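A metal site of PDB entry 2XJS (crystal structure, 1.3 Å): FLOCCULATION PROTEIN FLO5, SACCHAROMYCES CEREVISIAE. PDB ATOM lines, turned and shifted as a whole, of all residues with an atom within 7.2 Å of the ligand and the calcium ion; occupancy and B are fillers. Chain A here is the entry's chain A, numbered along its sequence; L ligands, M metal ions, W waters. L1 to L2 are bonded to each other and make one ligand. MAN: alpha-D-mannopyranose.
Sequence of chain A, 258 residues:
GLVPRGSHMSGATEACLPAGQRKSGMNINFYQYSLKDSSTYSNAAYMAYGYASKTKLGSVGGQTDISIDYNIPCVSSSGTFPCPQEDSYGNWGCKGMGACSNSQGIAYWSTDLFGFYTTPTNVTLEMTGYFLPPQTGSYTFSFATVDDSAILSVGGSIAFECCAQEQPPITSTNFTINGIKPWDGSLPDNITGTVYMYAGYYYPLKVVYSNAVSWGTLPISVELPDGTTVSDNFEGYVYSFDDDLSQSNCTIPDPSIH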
ATOM      1  N   LYS A  36      23.415  -1.680  21.915  1.00  0.00           N
ATOM      2  CA  LYS A  36      24.841  -1.992  22.154  1.00  0.00           C
ATOM      3  C   LYS A  36      25.371  -3.223  21.423  1.00  0.00           C
ATOM      4  O   LYS A  36      26.448  -3.709  21.742  1.00  0.00           O
ATOM      5  CB  LYS A  36      25.179  -1.958  23.648  1.00  0.00           C
ATOM      6  CG  LYS A  36      25.076  -0.549  24.236  1.00  0.00           C
ATOM      7  CD  LYS A  36      25.249  -0.370  25.735  1.00  0.00           C
ATOM      8  CE  LYS A  36      24.101  -1.045  26.456  1.00  0.00           C
ATOM      9  NZ  LYS A  36      24.048  -0.751  27.896  1.00  0.00           N
ATOM     10  N   SER A  38      27.362  -4.243  18.748  1.00  0.00           N
ATOM     11  CA  SER A  38      28.358  -3.624  17.880  1.00  0.00           C
ATOM     12  C   SER A  38      28.925  -4.553  16.813  1.00  0.00           C
ATOM     13  O   SER A  38      29.951  -4.182  16.211  1.00  0.00           O
ATOM     14  CB  SER A  38      29.533  -3.114  18.729  1.00  0.00           C
ATOM     15  OG  SER A  38      30.074  -4.104  19.576  1.00  0.00           O
ATOM     16  N   TYR A  41      25.685  -5.144  12.596  1.00  0.00           N
ATOM     17  CA  TYR A  41      25.724  -4.144  11.536  1.00  0.00           C
ATOM     18  C   TYR A  41      27.024  -4.031  10.761  1.00  0.00           C
ATOM     19  O   TYR A  41      27.158  -3.165   9.904  1.00  0.00           O
ATOM     20  CB  TYR A  41      25.299  -2.787  12.126  1.00  0.00           C
ATOM     21  CG  TYR A  41      26.138  -2.150  13.212  1.00  0.00           C
ATOM     22  CD1 TYR A  41      25.578  -1.214  14.067  1.00  0.00           C
ATOM     23  CD2 TYR A  41      27.471  -2.470  13.459  1.00  0.00           C
ATOM     24  CE1 TYR A  41      26.316  -0.610  15.082  1.00  0.00           C
ATOM     25  CE2 TYR A  41      28.222  -1.892  14.478  1.00  0.00           C
ATOM     26  CZ  TYR A  41      27.639  -0.930  15.296  1.00  0.00           C
ATOM     27  OH  TYR A  41      28.354  -0.317  16.312  1.00  0.00           O
ATOM     28  N   TYR A  70      20.159  12.447  15.120  1.00  0.00           N
ATOM     29  CA  TYR A  70      19.514  12.079  16.382  1.00  0.00           C
ATOM     30  C   TYR A  70      20.491  12.366  17.514  1.00  0.00           C
ATOM     31  O   TYR A  70      21.622  11.837  17.543  1.00  0.00           O
ATOM     32  CB  TYR A  70      19.154  10.578  16.394  1.00  0.00           C
ATOM     33  CG  TYR A  70      18.662  10.187  17.776  1.00  0.00           C
ATOM     34  CD1 TYR A  70      17.498  10.700  18.317  1.00  0.00           C
ATOM     35  CD2 TYR A  70      19.450   9.358  18.563  1.00  0.00           C
ATOM     36  CE1 TYR A  70      17.096  10.410  19.645  1.00  0.00           C
ATOM     37  CE2 TYR A  70      19.045   9.063  19.854  1.00  0.00           C
ATOM     38  CZ  TYR A  70      17.897   9.573  20.399  1.00  0.00           C
ATOM     39  OH  TYR A  70      17.552   9.275  21.690  1.00  0.00           O
ATOM     40  N   ILE A  72      20.720  12.288  21.811  1.00  0.00           N
ATOM     41  CA  ILE A  72      20.143  11.790  23.030  1.00  0.00           C
ATOM     42  C   ILE A  72      19.767  12.924  23.997  1.00  0.00           C
ATOM     43  O   ILE A  72      20.345  14.023  23.939  1.00  0.00           O
ATOM     44  CB  ILE A  72      21.033  10.757  23.760  1.00  0.00           C
ATOM     45  CG1 ILE A  72      22.415  11.299  24.123  1.00  0.00           C
ATOM     46  CG2 ILE A  72      21.132   9.421  22.973  1.00  0.00           C
ATOM     47  CD1 ILE A  72      23.176  10.516  25.191  1.00  0.00           C
ATOM     48  N   GLN A  85      26.170  16.053  20.021  1.00  0.00           N
ATOM     49  CA  GLN A  85      27.258  15.222  20.529  1.00  0.00           C
ATOM     50  C   GLN A  85      28.520  16.046  20.807  1.00  0.00           C
ATOM     51  O   GLN A  85      29.249  15.785  21.758  1.00  0.00           O
ATOM     52  CB  GLN A  85      27.554  14.082  19.565  1.00  0.00           C
ATOM     53  CG  GLN A  85      28.509  13.021  20.138  1.00  0.00           C
ATOM     54  CD  GLN A  85      28.683  11.725  19.343  1.00  0.00           C
ATOM     55  OE1 GLN A  85      29.299  10.787  19.882  1.00  0.00           O
ATOM     56  NE2 GLN A  85      28.204  11.655  18.097  1.00  0.00           N
ATOM     57  N   SER A 103      21.740   8.163  31.799  1.00  0.00           N
ATOM     58  CA  SER A 103      22.776   7.351  31.169  1.00  0.00           C
ATOM     59  C   SER A 103      22.855   7.501  29.669  1.00  0.00           C
ATOM     60  O   SER A 103      21.844   7.511  28.982  1.00  0.00           O
ATOM     61  CB  SER A 103      22.521   5.877  31.473  1.00  0.00           C
ATOM     62  OG  SER A 103      23.479   5.014  30.858  1.00  0.00           O
ATOM     63  N   GLN A 104      24.048   7.579  29.105  1.00  0.00           N
ATOM     64  CA  GLN A 104      24.249   7.491  27.665  1.00  0.00           C
ATOM     65  C   GLN A 104      24.052   6.088  27.121  1.00  0.00           C
ATOM     66  O   GLN A 104      24.055   5.897  25.892  1.00  0.00           O
ATOM     67  CB  GLN A 104      25.637   7.973  27.276  1.00  0.00           C
ATOM     68  CG  GLN A 104      25.984   9.393  27.547  1.00  0.00           C
ATOM     69  CD  GLN A 104      27.304   9.847  26.911  1.00  0.00           C
ATOM     70  OE1 GLN A 104      27.870   9.156  26.070  1.00  0.00           O
ATOM     71  NE2 GLN A 104      27.753  11.046  27.257  1.00  0.00           N
ATOM     72  N   GLY A 105      23.919   5.080  27.977  1.00  0.00           N
ATOM     73  CA  GLY A 105      23.926   3.683  27.584  1.00  0.00           C
ATOM     74  C   GLY A 105      22.605   2.951  27.575  1.00  0.00           C
ATOM     75  O   GLY A 105      22.629   1.724  27.461  1.00  0.00           O
ATOM     76  N   ILE A 106      21.486   3.635  27.760  1.00  0.00           N
ATOM     77  CA  ILE A 106      20.147   3.051  27.725  1.00  0.00           C
ATOM     78  C   ILE A 106      19.453   3.394  26.424  1.00  0.00           C
ATOM     79  O   ILE A 106      19.870   4.317  25.702  1.00  0.00           O
ATOM     80  CB  ILE A 106      19.319   3.424  28.967  1.00  0.00           C
ATOM     81  CG1 ILE A 106      19.009   4.933  29.058  1.00  0.00           C
ATOM     82  CG2 ILE A 106      19.963   2.889  30.297  1.00  0.00           C
ATOM     83  CD1 ILE A 106      18.016   5.261  30.162  1.00  0.00           C
ATOM     84  N   PRO A 120      15.523   5.576  18.615  1.00  0.00           N
ATOM     85  CA  PRO A 120      16.559   5.957  17.648  1.00  0.00           C
ATOM     86  C   PRO A 120      17.959   5.536  18.066  1.00  0.00           C
ATOM     87  O   PRO A 120      18.858   5.543  17.236  1.00  0.00           O
ATOM     88  CB  PRO A 120      16.405   7.474  17.484  1.00  0.00           C
ATOM     89  CG  PRO A 120      15.013   7.688  17.833  1.00  0.00           C
ATOM     90  CD  PRO A 120      14.731   6.755  19.018  1.00  0.00           C
ATOM     91  N   THR A 121      18.145   5.282  19.355  1.00  0.00           N
ATOM     92  CA  THR A 121      19.384   4.734  19.901  1.00  0.00           C
ATOM     93  C   THR A 121      19.766   3.385  19.343  1.00  0.00           C
ATOM     94  O   THR A 121      20.933   3.029  19.386  1.00  0.00           O
ATOM     95  CB  THR A 121      19.265   4.602  21.448  1.00  0.00           C
ATOM     96  OG1 THR A 121      18.018   3.966  21.755  1.00  0.00           O
ATOM     97  CG2 THR A 121      19.290   5.941  22.155  1.00  0.00           C
ATOM     98  N   ASP A 147      27.221   7.275  11.753  1.00  0.00           N
ATOM     99  CA  ASP A 147      27.159   6.803  13.121  1.00  0.00           C
ATOM    100  C   ASP A 147      25.821   6.069  13.247  1.00  0.00           C
ATOM    101  O   ASP A 147      24.793   6.749  13.337  1.00  0.00           O
ATOM    102  CB  ASP A 147      27.314   7.949  14.118  1.00  0.00           C
ATOM    103  CG  ASP A 147      27.212   7.544  15.594  1.00  0.00           C
ATOM    104  OD1 ASP A 147      27.596   8.325  16.499  1.00  0.00           O
ATOM    105  OD2 ASP A 147      26.715   6.458  15.911  1.00  0.00           O
ATOM    106  N   ASP A 148      25.791   4.728  13.226  1.00  0.00           N
ATOM    107  CA  ASP A 148      26.920   3.778  13.282  1.00  0.00           C
ATOM    108  C   ASP A 148      27.292   3.101  11.955  1.00  0.00           C
ATOM    109  O   ASP A 148      28.496   2.927  11.732  1.00  0.00           O
ATOM    110  CB  ASP A 148      26.608   2.683  14.315  1.00  0.00           C
ATOM    111  CG  ASP A 148      26.825   3.165  15.736  1.00  0.00           C
ATOM    112  OD1 ASP A 148      28.000   3.426  16.143  1.00  0.00           O
ATOM    113  OD2 ASP A 148      25.829   3.321  16.484  1.00  0.00           O
ATOM    114  N   LYS A 181      30.154  -0.264   9.279  1.00  0.00           N
ATOM    115  CA  LYS A 181      31.100  -0.085  10.392  1.00  0.00           C
ATOM    116  C   LYS A 181      32.156  -1.187  10.329  1.00  0.00           C
ATOM    117  O   LYS A 181      31.796  -2.358  10.387  1.00  0.00           O
ATOM    118  CB  LYS A 181      30.351  -0.122  11.729  1.00  0.00           C
ATOM    119  CG  LYS A 181      31.238   0.271  12.924  1.00  0.00           C
ATOM    120  CD  LYS A 181      31.154   1.771  13.114  1.00  0.00           C
ATOM    121  CE  LYS A 181      32.309   2.452  13.774  1.00  0.00           C
ATOM    122  NZ  LYS A 181      32.408   3.877  13.292  1.00  0.00           N
ATOM    123  N   TYR A 209      20.437   2.092   7.181  1.00  0.00           N
ATOM    124  CA  TYR A 209      21.106   2.796   8.271  1.00  0.00           C
ATOM    125  C   TYR A 209      20.856   2.106   9.601  1.00  0.00           C
ATOM    126  O   TYR A 209      19.741   1.711   9.872  1.00  0.00           O
ATOM    127  CB  TYR A 209      20.526   4.247   8.341  1.00  0.00           C
ATOM    128  CG  TYR A 209      20.924   4.919   9.647  1.00  0.00           C
ATOM    129  CD1 TYR A 209      22.225   5.439   9.818  1.00  0.00           C
ATOM    130  CD2 TYR A 209      20.096   4.920  10.750  1.00  0.00           C
ATOM    131  CE1 TYR A 209      22.633   5.934  11.020  1.00  0.00           C
ATOM    132  CE2 TYR A 209      20.511   5.419  11.975  1.00  0.00           C
ATOM    133  CZ  TYR A 209      21.781   5.943  12.123  1.00  0.00           C
ATOM    134  OH  TYR A 209      22.145   6.422  13.346  1.00  0.00           O
ATOM    135  N   SER A 210      21.916   1.961  10.416  1.00  0.00           N
ATOM    136  CA  SER A 210      21.764   1.374  11.737  1.00  0.00           C
ATOM    137  C   SER A 210      22.471   2.212  12.808  1.00  0.00           C
ATOM    138  O   SER A 210      23.562   2.763  12.590  1.00  0.00           O
ATOM    139  CB  SER A 210      22.227  -0.079  11.698  1.00  0.00           C
ATOM    140  OG  SER A 210      21.899  -0.785  12.873  1.00  0.00           O
ATOM    141  N   ASN A 211      21.832   2.273  13.964  1.00  0.00           N
ATOM    142  CA  ASN A 211      22.392   2.826  15.197  1.00  0.00           C
ATOM    143  C   ASN A 211      22.314   1.751  16.270  1.00  0.00           C
ATOM    144  O   ASN A 211      21.272   1.096  16.371  1.00  0.00           O
ATOM    145  CB  ASN A 211      21.635   4.076  15.646  1.00  0.00           C
ATOM    146  CG  ASN A 211      22.391   4.870  16.689  1.00  0.00           C
ATOM    147  OD1 ASN A 211      23.589   4.706  16.852  1.00  0.00           O
ATOM    148  ND2 ASN A 211      21.675   5.757  17.366  1.00  0.00           N
ATOM    149  N   ALA A 212      23.393   1.580  17.040  1.00  0.00           N
ATOM    150  CA  ALA A 212      23.437   0.647  18.150  1.00  0.00           C
ATOM    151  C   ALA A 212      23.367   1.289  19.523  1.00  0.00           C
ATOM    152  O   ALA A 212      22.956   0.662  20.509  1.00  0.00           O
ATOM    153  CB  ALA A 212      24.713  -0.200  18.143  1.00  0.00           C
ATOM    154  N   VAL A 213      23.798   2.549  19.648  1.00  0.00           N
ATOM    155  CA  VAL A 213      23.772   3.216  20.934  1.00  0.00           C
ATOM    156  C   VAL A 213      23.818   4.730  20.693  1.00  0.00           C
ATOM    157  O   VAL A 213      24.392   5.239  19.728  1.00  0.00           O
ATOM    158  CB  VAL A 213      24.887   2.740  21.845  1.00  0.00           C
ATOM    159  CG1 VAL A 213      26.235   3.218  21.352  1.00  0.00           C
ATOM    160  CG2 VAL A 213      24.675   3.072  23.317  1.00  0.00           C
ATOM    161  N   SER A 214      23.246   5.438  21.663  1.00  0.00           N
ATOM    162  CA  SER A 214      23.267   6.889  21.766  1.00  0.00           C
ATOM    163  C   SER A 214      23.081   7.613  20.417  1.00  0.00           C
ATOM    164  O   SER A 214      22.029   7.430  19.790  1.00  0.00           O
ATOM    165  CB  SER A 214      24.451   7.377  22.613  1.00  0.00           C
ATOM    166  OG  SER A 214      25.704   7.109  21.996  1.00  0.00           O
ATOM    167  N   TRP A 215      23.988   8.504  20.048  1.00  0.00           N
ATOM    168  CA  TRP A 215      23.781   9.389  18.904  1.00  0.00           C
ATOM    169  C   TRP A 215      23.681   8.639  17.589  1.00  0.00           C
ATOM    170  O   TRP A 215      24.278   7.574  17.434  1.00  0.00           O
ATOM    171  CB  TRP A 215      24.937  10.419  18.829  1.00  0.00           C
ATOM    172  CG  TRP A 215      24.871  11.462  19.894  1.00  0.00           C
ATOM    173  CD1 TRP A 215      24.235  12.655  19.785  1.00  0.00           C
ATOM    174  CD2 TRP A 215      25.437  11.450  21.220  1.00  0.00           C
ATOM    175  NE1 TRP A 215      24.344  13.378  20.930  1.00  0.00           N
ATOM    176  CE2 TRP A 215      25.107  12.672  21.824  1.00  0.00           C
ATOM    177  CE3 TRP A 215      26.222  10.539  21.920  1.00  0.00           C
ATOM    178  CZ2 TRP A 215      25.492  12.994  23.125  1.00  0.00           C
ATOM    179  CZ3 TRP A 215      26.638  10.885  23.233  1.00  0.00           C
ATOM    180  CH2 TRP A 215      26.261  12.116  23.789  1.00  0.00           C
ATOM    181  N   GLY A 216      22.906   9.204  16.677  1.00  0.00           N
ATOM    182  CA  GLY A 216      22.783   8.663  15.321  1.00  0.00           C
ATOM    183  C   GLY A 216      22.985   9.750  14.313  1.00  0.00           C
ATOM    184  O   GLY A 216      22.337  10.797  14.442  1.00  0.00           O
ATOM    185  N   THR A 217      23.812   9.530  13.290  1.00  0.00           N
ATOM    186  CA  THR A 217      24.127  10.609  12.353  1.00  0.00           C
ATOM    187  C   THR A 217      24.360  10.023  10.947  1.00  0.00           C
ATOM    188  O   THR A 217      25.141   9.078  10.759  1.00  0.00           O
ATOM    189  CB  THR A 217      25.398  11.374  12.799  1.00  0.00           C
ATOM    190  OG1 THR A 217      25.344  11.646  14.205  1.00  0.00           O
ATOM    191  CG2 THR A 217      25.470  12.728  12.091  1.00  0.00           C
HETATM  192  C1  MAN L   1      30.516   5.089  23.821  1.00  0.00           C
HETATM  193  C2  MAN L   1      29.549   6.268  23.606  1.00  0.00           C
HETATM  194  C3  MAN L   1      28.345   6.231  24.572  1.00  0.00           C
HETATM  195  C4  MAN L   1      27.736   4.826  24.631  1.00  0.00           C
HETATM  196  C5  MAN L   1      28.797   3.749  24.873  1.00  0.00           C
HETATM  197  C6  MAN L   1      28.217   2.348  24.888  1.00  0.00           C
HETATM  198  O1  MAN L   1      31.235   5.440  24.987  1.00  0.00           O
HETATM  199  O2  MAN L   1      28.975   6.174  22.289  1.00  0.00           O
HETATM  200  O3  MAN L   1      27.373   7.193  24.239  1.00  0.00           O
HETATM  201  O4  MAN L   1      26.814   4.741  25.691  1.00  0.00           O
HETATM  202  O5  MAN L   1      29.789   3.860  23.835  1.00  0.00           O
HETATM  203  O6  MAN L   1      29.191   1.416  25.306  1.00  0.00           O
HETATM  204  C1  MAN L   2      29.774   6.729  21.227  1.00  0.00           C
HETATM  205  C2  MAN L   2      28.829   7.554  20.344  1.00  0.00           C
HETATM  206  C3  MAN L   2      27.832   6.590  19.720  1.00  0.00           C
HETATM  207  C4  MAN L   2      28.498   5.454  18.961  1.00  0.00           C
HETATM  208  C5  MAN L   2      29.444   4.741  19.935  1.00  0.00           C
HETATM  209  C6  MAN L   2      30.249   3.641  19.271  1.00  0.00           C
HETATM  210  O2  MAN L   2      29.555   8.190  19.315  1.00  0.00           O
HETATM  211  O3  MAN L   2      26.877   7.254  18.960  1.00  0.00           O
HETATM  212  O4  MAN L   2      27.520   4.567  18.450  1.00  0.00           O
HETATM  213  O5  MAN L   2      30.364   5.678  20.492  1.00  0.00           O
HETATM  214  O6  MAN L   2      31.058   4.193  18.263  1.00  0.00           O
HETATM  215 CA    CA M   1      25.561   5.649  17.688  1.00  0.00          CA
HETATM  216  O   HOH W   1      27.468   4.249  28.407  1.00  0.00           O
HETATM  217  O   HOH W   2      30.314   2.605  16.147  1.00  0.00           O
HETATM  218  O   HOH W   3      28.836  -1.266  24.785  1.00  0.00           O
HETATM  219  O   HOH W   4      33.538   4.357  20.713  1.00  0.00           O
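The backbone NH (N) of Trp 215 sits close to an oxygen (O3) of MAN L2 (3.3 Å).
O2 of MAN L2 is in hydrogen-bond range of OE1 of Gln 85, at 2.7 Å.
O of Gln 104 lies within hydrogen-bond range of O4 of MAN L1, at 3.0 Å.
The side-chain amide oxygen (OE1) of Gln 104 sits at hydrogen-bond distance from an oxygen (O3) of MAN L1, at 2.7 Å.
The side-chain hydroxyl of Ser 214 sits at hydrogen-bond distance from an oxygen (O3) of MAN L1.
Water W2 lies within hydrogen-bond range of OD1 of Asp 148 (2.5 Å) and O6 of MAN L2 (2.7 Å).
The calcium ion is bound by the side-chain carboxylate of Asp 147 (2.3 Å), the backbone carbonyl oxygen of Trp 215 (2.3 Å), the side-chain amide oxygen of Asn 211 (2.3 Å), an oxygen (O4) of MAN L2 (2.4 Å), the backbone carbonyl oxygen of Val 213 (2.4 Å), an oxygen (O3) of MAN L2 (2.4 Å) and the side-chain carboxylate of Asp 148 (2.6 Å).
Five residues have an atom within 4 Å of the calcium ion: Asp 147, Asp 148, Asn 211, Val 213 and Trp 215.
O of Asp 147 sits at hydrogen-bond distance from OH of Tyr 209.
The backbone carbonyl oxygen (O) of Ser 214 is in hydrogen-bond range of the side-chain amide nitrogen (ND2) of Asn 211 (3.0 Å).
ND2 of Asn 211 sits at hydrogen-bond distance from O of Thr 121.
The side-chain amide nitrogen (ND2) of Asn 211 sits at hydrogen-bond distance from the backbone carbonyl oxygen (O) of Pro 120 (2.8 Å).
O of Thr 121 lies within hydrogen-bond range of N of Val 213 (2.9 Å).
N of Ala 212 sits close to OD2 of Asp 148, 3.0 Å away.
N of Asp 148 sits at hydrogen-bond distance from O of Ser 210 (3.0 Å).
The backbone NH of Gly 105 sits at hydrogen-bond distance from the side-chain hydroxyl of Ser 103, 2.9 Å away.
Gly 105 touches the ligand.
Of the 24 residues printed, 8 come within 4 Å of the ligand.
The nearest printed residue that does not touch the ligand is Lys 36 (4.1 Å).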
